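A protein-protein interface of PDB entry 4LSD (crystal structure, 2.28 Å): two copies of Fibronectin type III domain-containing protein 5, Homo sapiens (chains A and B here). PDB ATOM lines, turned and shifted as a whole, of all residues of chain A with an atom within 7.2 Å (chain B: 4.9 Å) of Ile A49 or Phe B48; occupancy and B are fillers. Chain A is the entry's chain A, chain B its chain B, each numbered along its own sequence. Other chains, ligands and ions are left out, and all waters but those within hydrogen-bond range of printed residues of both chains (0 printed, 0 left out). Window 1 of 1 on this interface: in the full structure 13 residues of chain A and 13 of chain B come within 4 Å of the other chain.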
ATOM      1  N   PHE A  34     -22.735  14.772  -7.811  1.00  0.00           N
ATOM      2  CA  PHE A  34     -21.589  15.646  -7.957  1.00  0.00           C
ATOM      3  C   PHE A  34     -20.835  15.826  -6.648  1.00  0.00           C
ATOM      4  O   PHE A  34     -21.386  15.631  -5.569  1.00  0.00           O
ATOM      5  CB  PHE A  34     -22.063  17.011  -8.414  1.00  0.00           C
ATOM      6  CG  PHE A  34     -22.704  17.823  -7.318  1.00  0.00           C
ATOM      7  CD1 PHE A  34     -21.922  18.577  -6.442  1.00  0.00           C
ATOM      8  CD2 PHE A  34     -24.085  17.830  -7.155  1.00  0.00           C
ATOM      9  CE1 PHE A  34     -22.503  19.325  -5.424  1.00  0.00           C
ATOM     10  CE2 PHE A  34     -24.683  18.576  -6.137  1.00  0.00           C
ATOM     11  CZ  PHE A  34     -23.891  19.326  -5.270  1.00  0.00           C
ATOM     12  N   ALA A  35     -19.571  16.218  -6.749  1.00  0.00           N
ATOM     13  CA  ALA A  35     -18.759  16.486  -5.569  1.00  0.00           C
ATOM     14  C   ALA A  35     -18.089  17.822  -5.829  1.00  0.00           C
ATOM     15  O   ALA A  35     -17.528  18.047  -6.900  1.00  0.00           O
ATOM     16  CB  ALA A  35     -17.721  15.404  -5.368  1.00  0.00           C
ATOM     17  N   ILE A  36     -18.169  18.723  -4.860  1.00  0.00           N
ATOM     18  CA  ILE A  36     -17.553  20.043  -4.996  1.00  0.00           C
ATOM     19  C   ILE A  36     -16.530  20.275  -3.878  1.00  0.00           C
ATOM     20  O   ILE A  36     -16.708  19.796  -2.754  1.00  0.00           O
ATOM     21  CB  ILE A  36     -18.618  21.179  -4.955  1.00  0.00           C
ATOM     22  CG1 ILE A  36     -19.203  21.407  -6.348  1.00  0.00           C
ATOM     23  CG2 ILE A  36     -18.001  22.475  -4.459  1.00  0.00           C
ATOM     24  CD1 ILE A  36     -20.138  22.607  -6.429  1.00  0.00           C
ATOM     25  N   SER A  37     -15.453  20.992  -4.206  1.00  0.00           N
ATOM     26  CA  SER A  37     -14.397  21.336  -3.247  1.00  0.00           C
ATOM     27  C   SER A  37     -14.350  22.835  -3.207  1.00  0.00           C
ATOM     28  O   SER A  37     -14.419  23.495  -4.243  1.00  0.00           O
ATOM     29  CB  SER A  37     -13.010  20.874  -3.693  1.00  0.00           C
ATOM     30  OG  SER A  37     -12.943  19.476  -3.850  1.00  0.00           O
ATOM     31  N   GLN A  38     -14.205  23.371  -2.008  1.00  0.00           N
ATOM     32  CA  GLN A  38     -14.140  24.808  -1.836  1.00  0.00           C
ATOM     33  C   GLN A  38     -13.038  25.174  -0.862  1.00  0.00           C
ATOM     34  O   GLN A  38     -12.917  24.580   0.207  1.00  0.00           O
ATOM     35  CB  GLN A  38     -15.471  25.331  -1.299  1.00  0.00           C
ATOM     36  CG  GLN A  38     -15.416  26.775  -0.813  1.00  0.00           C
ATOM     37  CD  GLN A  38     -16.577  27.127   0.100  1.00  0.00           C
ATOM     38  OE1 GLN A  38     -17.748  26.956  -0.257  1.00  0.00           O
ATOM     39  NE2 GLN A  38     -16.258  27.623   1.290  1.00  0.00           N
ATOM     40  N   ARG A  47     -13.820  23.023   2.457  1.00  0.00           N
ATOM     41  CA  ARG A  47     -15.203  22.562   2.502  1.00  0.00           C
ATOM     42  C   ARG A  47     -15.531  21.648   1.323  1.00  0.00           C
ATOM     43  O   ARG A  47     -15.200  21.952   0.175  1.00  0.00           O
ATOM     44  CB  ARG A  47     -16.157  23.756   2.509  1.00  0.00           C
ATOM     45  CG  ARG A  47     -17.613  23.364   2.635  1.00  0.00           C
ATOM     46  CD  ARG A  47     -18.425  24.468   3.303  1.00  0.00           C
ATOM     47  NE  ARG A  47     -18.984  25.401   2.334  1.00  0.00           N
ATOM     48  CZ  ARG A  47     -19.349  26.647   2.618  1.00  0.00           C
ATOM     49  NH1 ARG A  47     -19.205  27.121   3.852  1.00  0.00           N
ATOM     50  NH2 ARG A  47     -19.873  27.413   1.664  1.00  0.00           N
ATOM     51  N   PHE A  48     -16.183  20.525   1.618  1.00  0.00           N
ATOM     52  CA  PHE A  48     -16.557  19.558   0.592  1.00  0.00           C
ATOM     53  C   PHE A  48     -18.058  19.262   0.600  1.00  0.00           C
ATOM     54  O   PHE A  48     -18.615  18.931   1.644  1.00  0.00           O
ATOM     55  CB  PHE A  48     -15.815  18.235   0.800  1.00  0.00           C
ATOM     56  CG  PHE A  48     -14.331  18.377   0.880  1.00  0.00           C
ATOM     57  CD1 PHE A  48     -13.697  18.573   2.108  1.00  0.00           C
ATOM     58  CD2 PHE A  48     -13.561  18.328  -0.279  1.00  0.00           C
ATOM     59  CE1 PHE A  48     -12.312  18.720   2.177  1.00  0.00           C
ATOM     60  CE2 PHE A  48     -12.181  18.474  -0.223  1.00  0.00           C
ATOM     61  CZ  PHE A  48     -11.551  18.671   1.004  1.00  0.00           C
ATOM     62  N   ILE A  49     -18.707  19.369  -0.558  1.00  0.00           N
ATOM     63  CA  ILE A  49     -20.128  19.070  -0.655  1.00  0.00           C
ATOM     64  C   ILE A  49     -20.324  17.997  -1.700  1.00  0.00           C
ATOM     65  O   ILE A  49     -19.747  18.064  -2.774  1.00  0.00           O
ATOM     66  CB  ILE A  49     -20.954  20.272  -1.087  1.00  0.00           C
ATOM     67  CG1 ILE A  49     -20.766  21.425  -0.106  1.00  0.00           C
ATOM     68  CG2 ILE A  49     -22.425  19.875  -1.140  1.00  0.00           C
ATOM     69  CD1 ILE A  49     -21.395  22.713  -0.569  1.00  0.00           C
ATOM     70  N   GLN A  50     -21.129  16.993  -1.380  1.00  0.00           N
ATOM     71  CA  GLN A  50     -21.407  15.913  -2.324  1.00  0.00           C
ATOM     72  C   GLN A  50     -22.904  15.638  -2.262  1.00  0.00           C
ATOM     73  O   GLN A  50     -23.505  15.714  -1.200  1.00  0.00           O
ATOM     74  CB  GLN A  50     -20.639  14.634  -1.954  1.00  0.00           C
ATOM     75  CG  GLN A  50     -20.772  13.517  -2.977  1.00  0.00           C
ATOM     76  CD  GLN A  50     -20.356  12.145  -2.442  1.00  0.00           C
ATOM     77  OE1 GLN A  50     -21.148  11.439  -1.807  1.00  0.00           O
ATOM     78  NE2 GLN A  50     -19.107  11.768  -2.693  1.00  0.00           N
ATOM     79  N   GLU A  51     -23.516  15.377  -3.407  1.00  0.00           N
ATOM     80  CA  GLU A  51     -24.934  15.048  -3.456  1.00  0.00           C
ATOM     81  C   GLU A  51     -25.041  13.963  -4.492  1.00  0.00           C
ATOM     82  O   GLU A  51     -24.436  14.042  -5.552  1.00  0.00           O
ATOM     83  CB  GLU A  51     -25.800  16.249  -3.849  1.00  0.00           C
ATOM     84  CG  GLU A  51     -25.906  17.306  -2.767  1.00  0.00           C
ATOM     85  CD  GLU A  51     -26.951  18.361  -3.080  1.00  0.00           C
ATOM     86  OE1 GLU A  51     -27.397  18.415  -4.245  1.00  0.00           O
ATOM     87  OE2 GLU A  51     -27.321  19.137  -2.168  1.00  0.00           O
ATOM     88  N   VAL A  52     -25.799  12.930  -4.171  1.00  0.00           N
ATOM     89  CA  VAL A  52     -25.958  11.811  -5.072  1.00  0.00           C
ATOM     90  C   VAL A  52     -27.447  11.513  -5.215  1.00  0.00           C
ATOM     91  O   VAL A  52     -28.252  11.934  -4.377  1.00  0.00           O
ATOM     92  CB  VAL A  52     -25.159  10.607  -4.521  1.00  0.00           C
ATOM     93  CG1 VAL A  52     -25.520   9.325  -5.237  1.00  0.00           C
ATOM     94  CG2 VAL A  52     -23.668  10.892  -4.693  1.00  0.00           C
ATOM     95  N   CYS A  59     -25.152  24.143  -7.099  1.00  0.00           N
ATOM     96  CA  CYS A  59     -24.923  23.938  -5.696  1.00  0.00           C
ATOM     97  C   CYS A  59     -24.611  25.273  -5.050  1.00  0.00           C
ATOM     98  O   CYS A  59     -23.721  25.987  -5.500  1.00  0.00           O
ATOM     99  CB  CYS A  59     -23.748  22.988  -5.534  1.00  0.00           C
ATOM    100  SG  CYS A  59     -23.178  22.811  -3.852  1.00  0.00           S
ATOM    101  N   ALA A  60     -25.342  25.605  -3.992  1.00  0.00           N
ATOM    102  CA  ALA A  60     -25.134  26.860  -3.274  1.00  0.00           C
ATOM    103  C   ALA A  60     -23.997  26.747  -2.263  1.00  0.00           C
ATOM    104  O   ALA A  60     -23.799  25.698  -1.662  1.00  0.00           O
ATOM    105  CB  ALA A  60     -26.397  27.255  -2.558  1.00  0.00           C
ATOM    106  N   LEU A  61     -23.250  27.832  -2.084  1.00  0.00           N
ATOM    107  CA  LEU A  61     -22.157  27.872  -1.124  1.00  0.00           C
ATOM    108  C   LEU A  61     -22.538  28.982  -0.164  1.00  0.00           C
ATOM    109  O   LEU A  61     -22.725  30.130  -0.567  1.00  0.00           O
ATOM    110  CB  LEU A  61     -20.833  28.213  -1.814  1.00  0.00           C
ATOM    111  CG  LEU A  61     -20.487  27.336  -3.016  1.00  0.00           C
ATOM    112  CD1 LEU A  61     -19.392  28.018  -3.821  1.00  0.00           C
ATOM    113  CD2 LEU A  61     -20.054  25.949  -2.560  1.00  0.00           C
ATOM    114  N   TRP A  62     -22.642  28.639   1.109  1.00  0.00           N
ATOM    115  CA  TRP A  62     -23.041  29.595   2.122  1.00  0.00           C
ATOM    116  C   TRP A  62     -21.919  29.944   3.089  1.00  0.00           C
ATOM    117  O   TRP A  62     -20.867  29.310   3.097  1.00  0.00           O
ATOM    118  CB  TRP A  62     -24.190  28.999   2.913  1.00  0.00           C
ATOM    119  CG  TRP A  62     -23.757  27.781   3.697  1.00  0.00           C
ATOM    120  CD1 TRP A  62     -23.479  27.724   5.034  1.00  0.00           C
ATOM    121  CD2 TRP A  62     -23.486  26.462   3.177  1.00  0.00           C
ATOM    122  NE1 TRP A  62     -23.052  26.459   5.383  1.00  0.00           N
ATOM    123  CE2 TRP A  62     -23.048  25.668   4.267  1.00  0.00           C
ATOM    124  CE3 TRP A  62     -23.571  25.880   1.902  1.00  0.00           C
ATOM    125  CZ2 TRP A  62     -22.690  24.321   4.115  1.00  0.00           C
ATOM    126  CZ3 TRP A  62     -23.217  24.542   1.754  1.00  0.00           C
ATOM    127  CH2 TRP A  62     -22.783  23.778   2.857  1.00  0.00           C
ATOM    128  N   HIS A  73     -13.844  23.476  -7.306  1.00  0.00           N
ATOM    129  CA  HIS A  73     -13.680  22.471  -8.354  1.00  0.00           C
ATOM    130  C   HIS A  73     -14.904  21.584  -8.293  1.00  0.00           C
ATOM    131  O   HIS A  73     -15.371  21.233  -7.212  1.00  0.00           O
ATOM    132  CB  HIS A  73     -12.443  21.593  -8.138  1.00  0.00           C
ATOM    133  CG  HIS A  73     -11.145  22.307  -8.346  1.00  0.00           C
ATOM    134  ND1 HIS A  73     -10.414  22.210  -9.506  1.00  0.00           N
ATOM    135  CD2 HIS A  73     -10.463  23.146  -7.531  1.00  0.00           C
ATOM    136  CE1 HIS A  73      -9.330  22.966  -9.402  1.00  0.00           C
ATOM    137  NE2 HIS A  73      -9.341  23.541  -8.217  1.00  0.00           N
ATOM    138  N   ALA B  35     -18.313  15.962   9.454  1.00  0.00           N
ATOM    139  CA  ALA B  35     -18.970  15.440   8.271  1.00  0.00           C
ATOM    140  C   ALA B  35     -20.434  15.304   8.661  1.00  0.00           C
ATOM    141  O   ALA B  35     -20.759  14.649   9.650  1.00  0.00           O
ATOM    142  CB  ALA B  35     -18.400  14.086   7.888  1.00  0.00           C
ATOM    143  N   ILE B  36     -21.308  15.957   7.905  1.00  0.00           N
ATOM    144  CA  ILE B  36     -22.736  15.896   8.170  1.00  0.00           C
ATOM    145  C   ILE B  36     -23.423  15.136   7.048  1.00  0.00           C
ATOM    146  O   ILE B  36     -23.167  15.387   5.872  1.00  0.00           O
ATOM    147  CB  ILE B  36     -23.404  17.288   8.222  1.00  0.00           C
ATOM    148  CG1 ILE B  36     -22.921  18.082   9.429  1.00  0.00           C
ATOM    149  CG2 ILE B  36     -24.923  17.124   8.311  1.00  0.00           C
ATOM    150  CD1 ILE B  36     -23.845  19.228   9.795  1.00  0.00           C
ATOM    151  N   SER B  37     -24.295  14.203   7.410  1.00  0.00           N
ATOM    152  CA  SER B  37     -25.050  13.442   6.423  1.00  0.00           C
ATOM    153  C   SER B  37     -26.468  14.058   6.483  1.00  0.00           C
ATOM    154  O   SER B  37     -26.963  14.341   7.576  1.00  0.00           O
ATOM    155  CB  SER B  37     -25.075  11.953   6.808  1.00  0.00           C
ATOM    156  OG  SER B  37     -25.975  11.231   5.980  1.00  0.00           O
ATOM    157  N   LEU B  46     -29.174  12.073  -1.560  1.00  0.00           N
ATOM    158  CA  LEU B  46     -28.316  11.914  -0.386  1.00  0.00           C
ATOM    159  C   LEU B  46     -27.260  13.024  -0.400  1.00  0.00           C
ATOM    160  O   LEU B  46     -26.460  13.123  -1.323  1.00  0.00           O
ATOM    161  CB  LEU B  46     -27.630  10.547  -0.429  1.00  0.00           C
ATOM    162  CG  LEU B  46     -28.591   9.410  -0.760  1.00  0.00           C
ATOM    163  CD1 LEU B  46     -27.839   8.100  -0.681  1.00  0.00           C
ATOM    164  CD2 LEU B  46     -29.765   9.409   0.211  1.00  0.00           C
ATOM    165  N   ARG B  47     -27.258  13.864   0.621  1.00  0.00           N
ATOM    166  CA  ARG B  47     -26.306  14.959   0.681  1.00  0.00           C
ATOM    167  C   ARG B  47     -25.261  14.731   1.769  1.00  0.00           C
ATOM    168  O   ARG B  47     -25.591  14.310   2.872  1.00  0.00           O
ATOM    169  CB  ARG B  47     -27.054  16.253   0.951  1.00  0.00           C
ATOM    170  CG  ARG B  47     -26.177  17.459   1.035  1.00  0.00           C
ATOM    171  CD  ARG B  47     -26.988  18.734   1.143  1.00  0.00           C
ATOM    172  NE  ARG B  47     -26.254  19.840   0.538  1.00  0.00           N
ATOM    173  CZ  ARG B  47     -26.207  21.061   1.048  1.00  0.00           C
ATOM    174  NH1 ARG B  47     -26.855  21.320   2.173  1.00  0.00           N
ATOM    175  NH2 ARG B  47     -25.513  22.017   0.444  1.00  0.00           N
ATOM    176  N   PHE B  48     -24.004  15.011   1.457  1.00  0.00           N
ATOM    177  CA  PHE B  48     -22.934  14.830   2.419  1.00  0.00           C
ATOM    178  C   PHE B  48     -22.031  16.057   2.434  1.00  0.00           C
ATOM    179  O   PHE B  48     -21.509  16.471   1.399  1.00  0.00           O
ATOM    180  CB  PHE B  48     -22.131  13.588   2.066  1.00  0.00           C
ATOM    181  CG  PHE B  48     -21.159  13.172   3.136  1.00  0.00           C
ATOM    182  CD1 PHE B  48     -19.835  12.865   2.811  1.00  0.00           C
ATOM    183  CD2 PHE B  48     -21.560  13.088   4.473  1.00  0.00           C
ATOM    184  CE1 PHE B  48     -18.922  12.479   3.795  1.00  0.00           C
ATOM    185  CE2 PHE B  48     -20.660  12.704   5.469  1.00  0.00           C
ATOM    186  CZ  PHE B  48     -19.335  12.400   5.130  1.00  0.00           C
ATOM    187  N   ILE B  49     -21.841  16.630   3.619  1.00  0.00           N
ATOM    188  CA  ILE B  49     -21.021  17.828   3.780  1.00  0.00           C
ATOM    189  C   ILE B  49     -19.855  17.628   4.750  1.00  0.00           C
ATOM    190  O   ILE B  49     -19.979  16.920   5.742  1.00  0.00           O
ATOM    191  CB  ILE B  49     -21.847  18.982   4.370  1.00  0.00           C
ATOM    192  CG1 ILE B  49     -23.088  19.237   3.535  1.00  0.00           C
ATOM    193  CG2 ILE B  49     -20.989  20.232   4.483  1.00  0.00           C
ATOM    194  CD1 ILE B  49     -24.127  20.038   4.289  1.00  0.00           C
ATOM    195  N   GLN B  50     -18.721  18.257   4.476  1.00  0.00           N
ATOM    196  CA  GLN B  50     -17.607  18.188   5.416  1.00  0.00           C
ATOM    197  C   GLN B  50     -16.731  19.425   5.361  1.00  0.00           C
ATOM    198  O   GLN B  50     -16.616  20.096   4.329  1.00  0.00           O
ATOM    199  CB  GLN B  50     -16.762  16.918   5.236  1.00  0.00           C
ATOM    200  CG  GLN B  50     -16.715  16.410   3.844  1.00  0.00           C
ATOM    201  CD  GLN B  50     -16.016  15.073   3.711  1.00  0.00           C
ATOM    202  OE1 GLN B  50     -15.183  14.684   4.544  1.00  0.00           O
ATOM    203  NE2 GLN B  50     -16.332  14.364   2.631  1.00  0.00           N
ATOM    204  N   GLN B  75     -20.478  13.469  12.121  1.00  0.00           N
ATOM    205  CA  GLN B  75     -19.294  12.674  12.318  1.00  0.00           C
ATOM    206  C   GLN B  75     -18.195  13.679  12.632  1.00  0.00           C
ATOM    207  O   GLN B  75     -18.164  14.751  12.046  1.00  0.00           O
ATOM    208  CB  GLN B  75     -19.029  11.949  11.011  1.00  0.00           C
ATOM    209  CG  GLN B  75     -17.964  10.900  11.000  1.00  0.00           C
ATOM    210  CD  GLN B  75     -18.156   9.937   9.833  1.00  0.00           C
ATOM    211  OE1 GLN B  75     -17.385   8.998   9.664  1.00  0.00           O
ATOM    212  NE2 GLN B  75     -19.198  10.162   9.034  1.00  0.00           N
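Ile A49 touches just one residue of chain B: Phe B48.
Of the printed residues of chain A, Phe B48 touches Phe A48, Ile A49 and Gln A50.
Of the printed residues of chain B, Trp A62 touches Arg B47 (3.7 Å).
Printed residues of chain A within 4 Å of Leu B46: Gln A50 (3.9 Å), Glu A51 (3.3 Å) and Val A52 (2.9 Å).
Of the printed residues of chain B, Arg A47 touches Gln B50 (3.4 Å).
Printed residues of chain A within 4 Å of Arg B47: Gln A50 (3.5 Å), Glu A51 (3.0 Å) and Trp A62 (3.7 Å).
Ile A36 touches none of the printed residues of chain B.
Ala B35 touches none of the printed residues of chain A.
The nearest residue of chain A that does not touch Phe B48 is Glu A51 (4.9 Å).
Arg A47 touches Gln B50, and with the chains exchanged Gln A50 touches Arg B47.
Phe A48 touches its own counterpart, Phe B48.
Phe A48 touches Ile B49, and with the chains exchanged Ile A49 touches Phe B48.
Phe A48 touches Gln B50, and with the chains exchanged Gln A50 touches Phe B48.
7 positions are printed for both chains.
Of the 12 pairs that touch across the chains among the printed residues, 7 have their exchanged pair printed and touching as well.
N of Phe A34 is in hydrogen-bond range of O of Glu A51, 2.9 Å away.
The backbone NH (N) of Ile A36 lies within hydrogen-bond range of the backbone carbonyl oxygen (O) of Ile A49 (2.7 Å).
The backbone NH of Gln A38 sits at hydrogen-bond distance from the backbone carbonyl oxygen of Arg A47, 2.8 Å away.
The backbone carbonyl oxygen (O) of Trp A62 is in hydrogen-bond range of the guanidinium group (NH2) of Arg A47 (2.6 Å).
The backbone carbonyl oxygen of Ile B49 is in hydrogen-bond range of the backbone NH of Ile B36 (2.7 Å).
Of the 9 printed residues of chain B, 5 touch a printed residue of chain A.
Hydrophobic or aromatic side chains of chain A within 4 Å of the printed part of chain B: Phe A48 and Trp A62.
Among the printed residues, Asp or Glu carboxylates within 4 Å of a Lys or Arg side-chain nitrogen of the other chain: Glu A51 with Arg B47 (3.0 Å).
Among the printed residues, merely in contact across the chains: Arg A47 with Gln B50 (3.4 Å), Phe A48 with Phe B48 (3.8 Å), Phe A48 with Ile B49 (3.4 Å), Ile A49 with Phe B48 (3.6 Å), Gln A50 with Leu B46 (3.9 Å), Gln A50 with Arg B47 (3.5 Å), Glu A51 with Leu B46 (3.3 Å) and Trp A62 with Arg B47 (3.7 Å).
The backbone NH of Phe A48 is in hydrogen-bond range of the backbone carbonyl oxygen of Gln B50.
The backbone carbonyl oxygen (O) of Gln A50 sits at hydrogen-bond distance from the backbone NH (N) of Phe B48, at 2.8 Å.
OE2 of Glu A51 lies within salt-bridge range of NE of Arg B47 (3.0 Å).
The backbone NH (N) of Val A52 sits at hydrogen-bond distance from the backbone carbonyl oxygen (O) of Leu B46 (2.9 Å).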
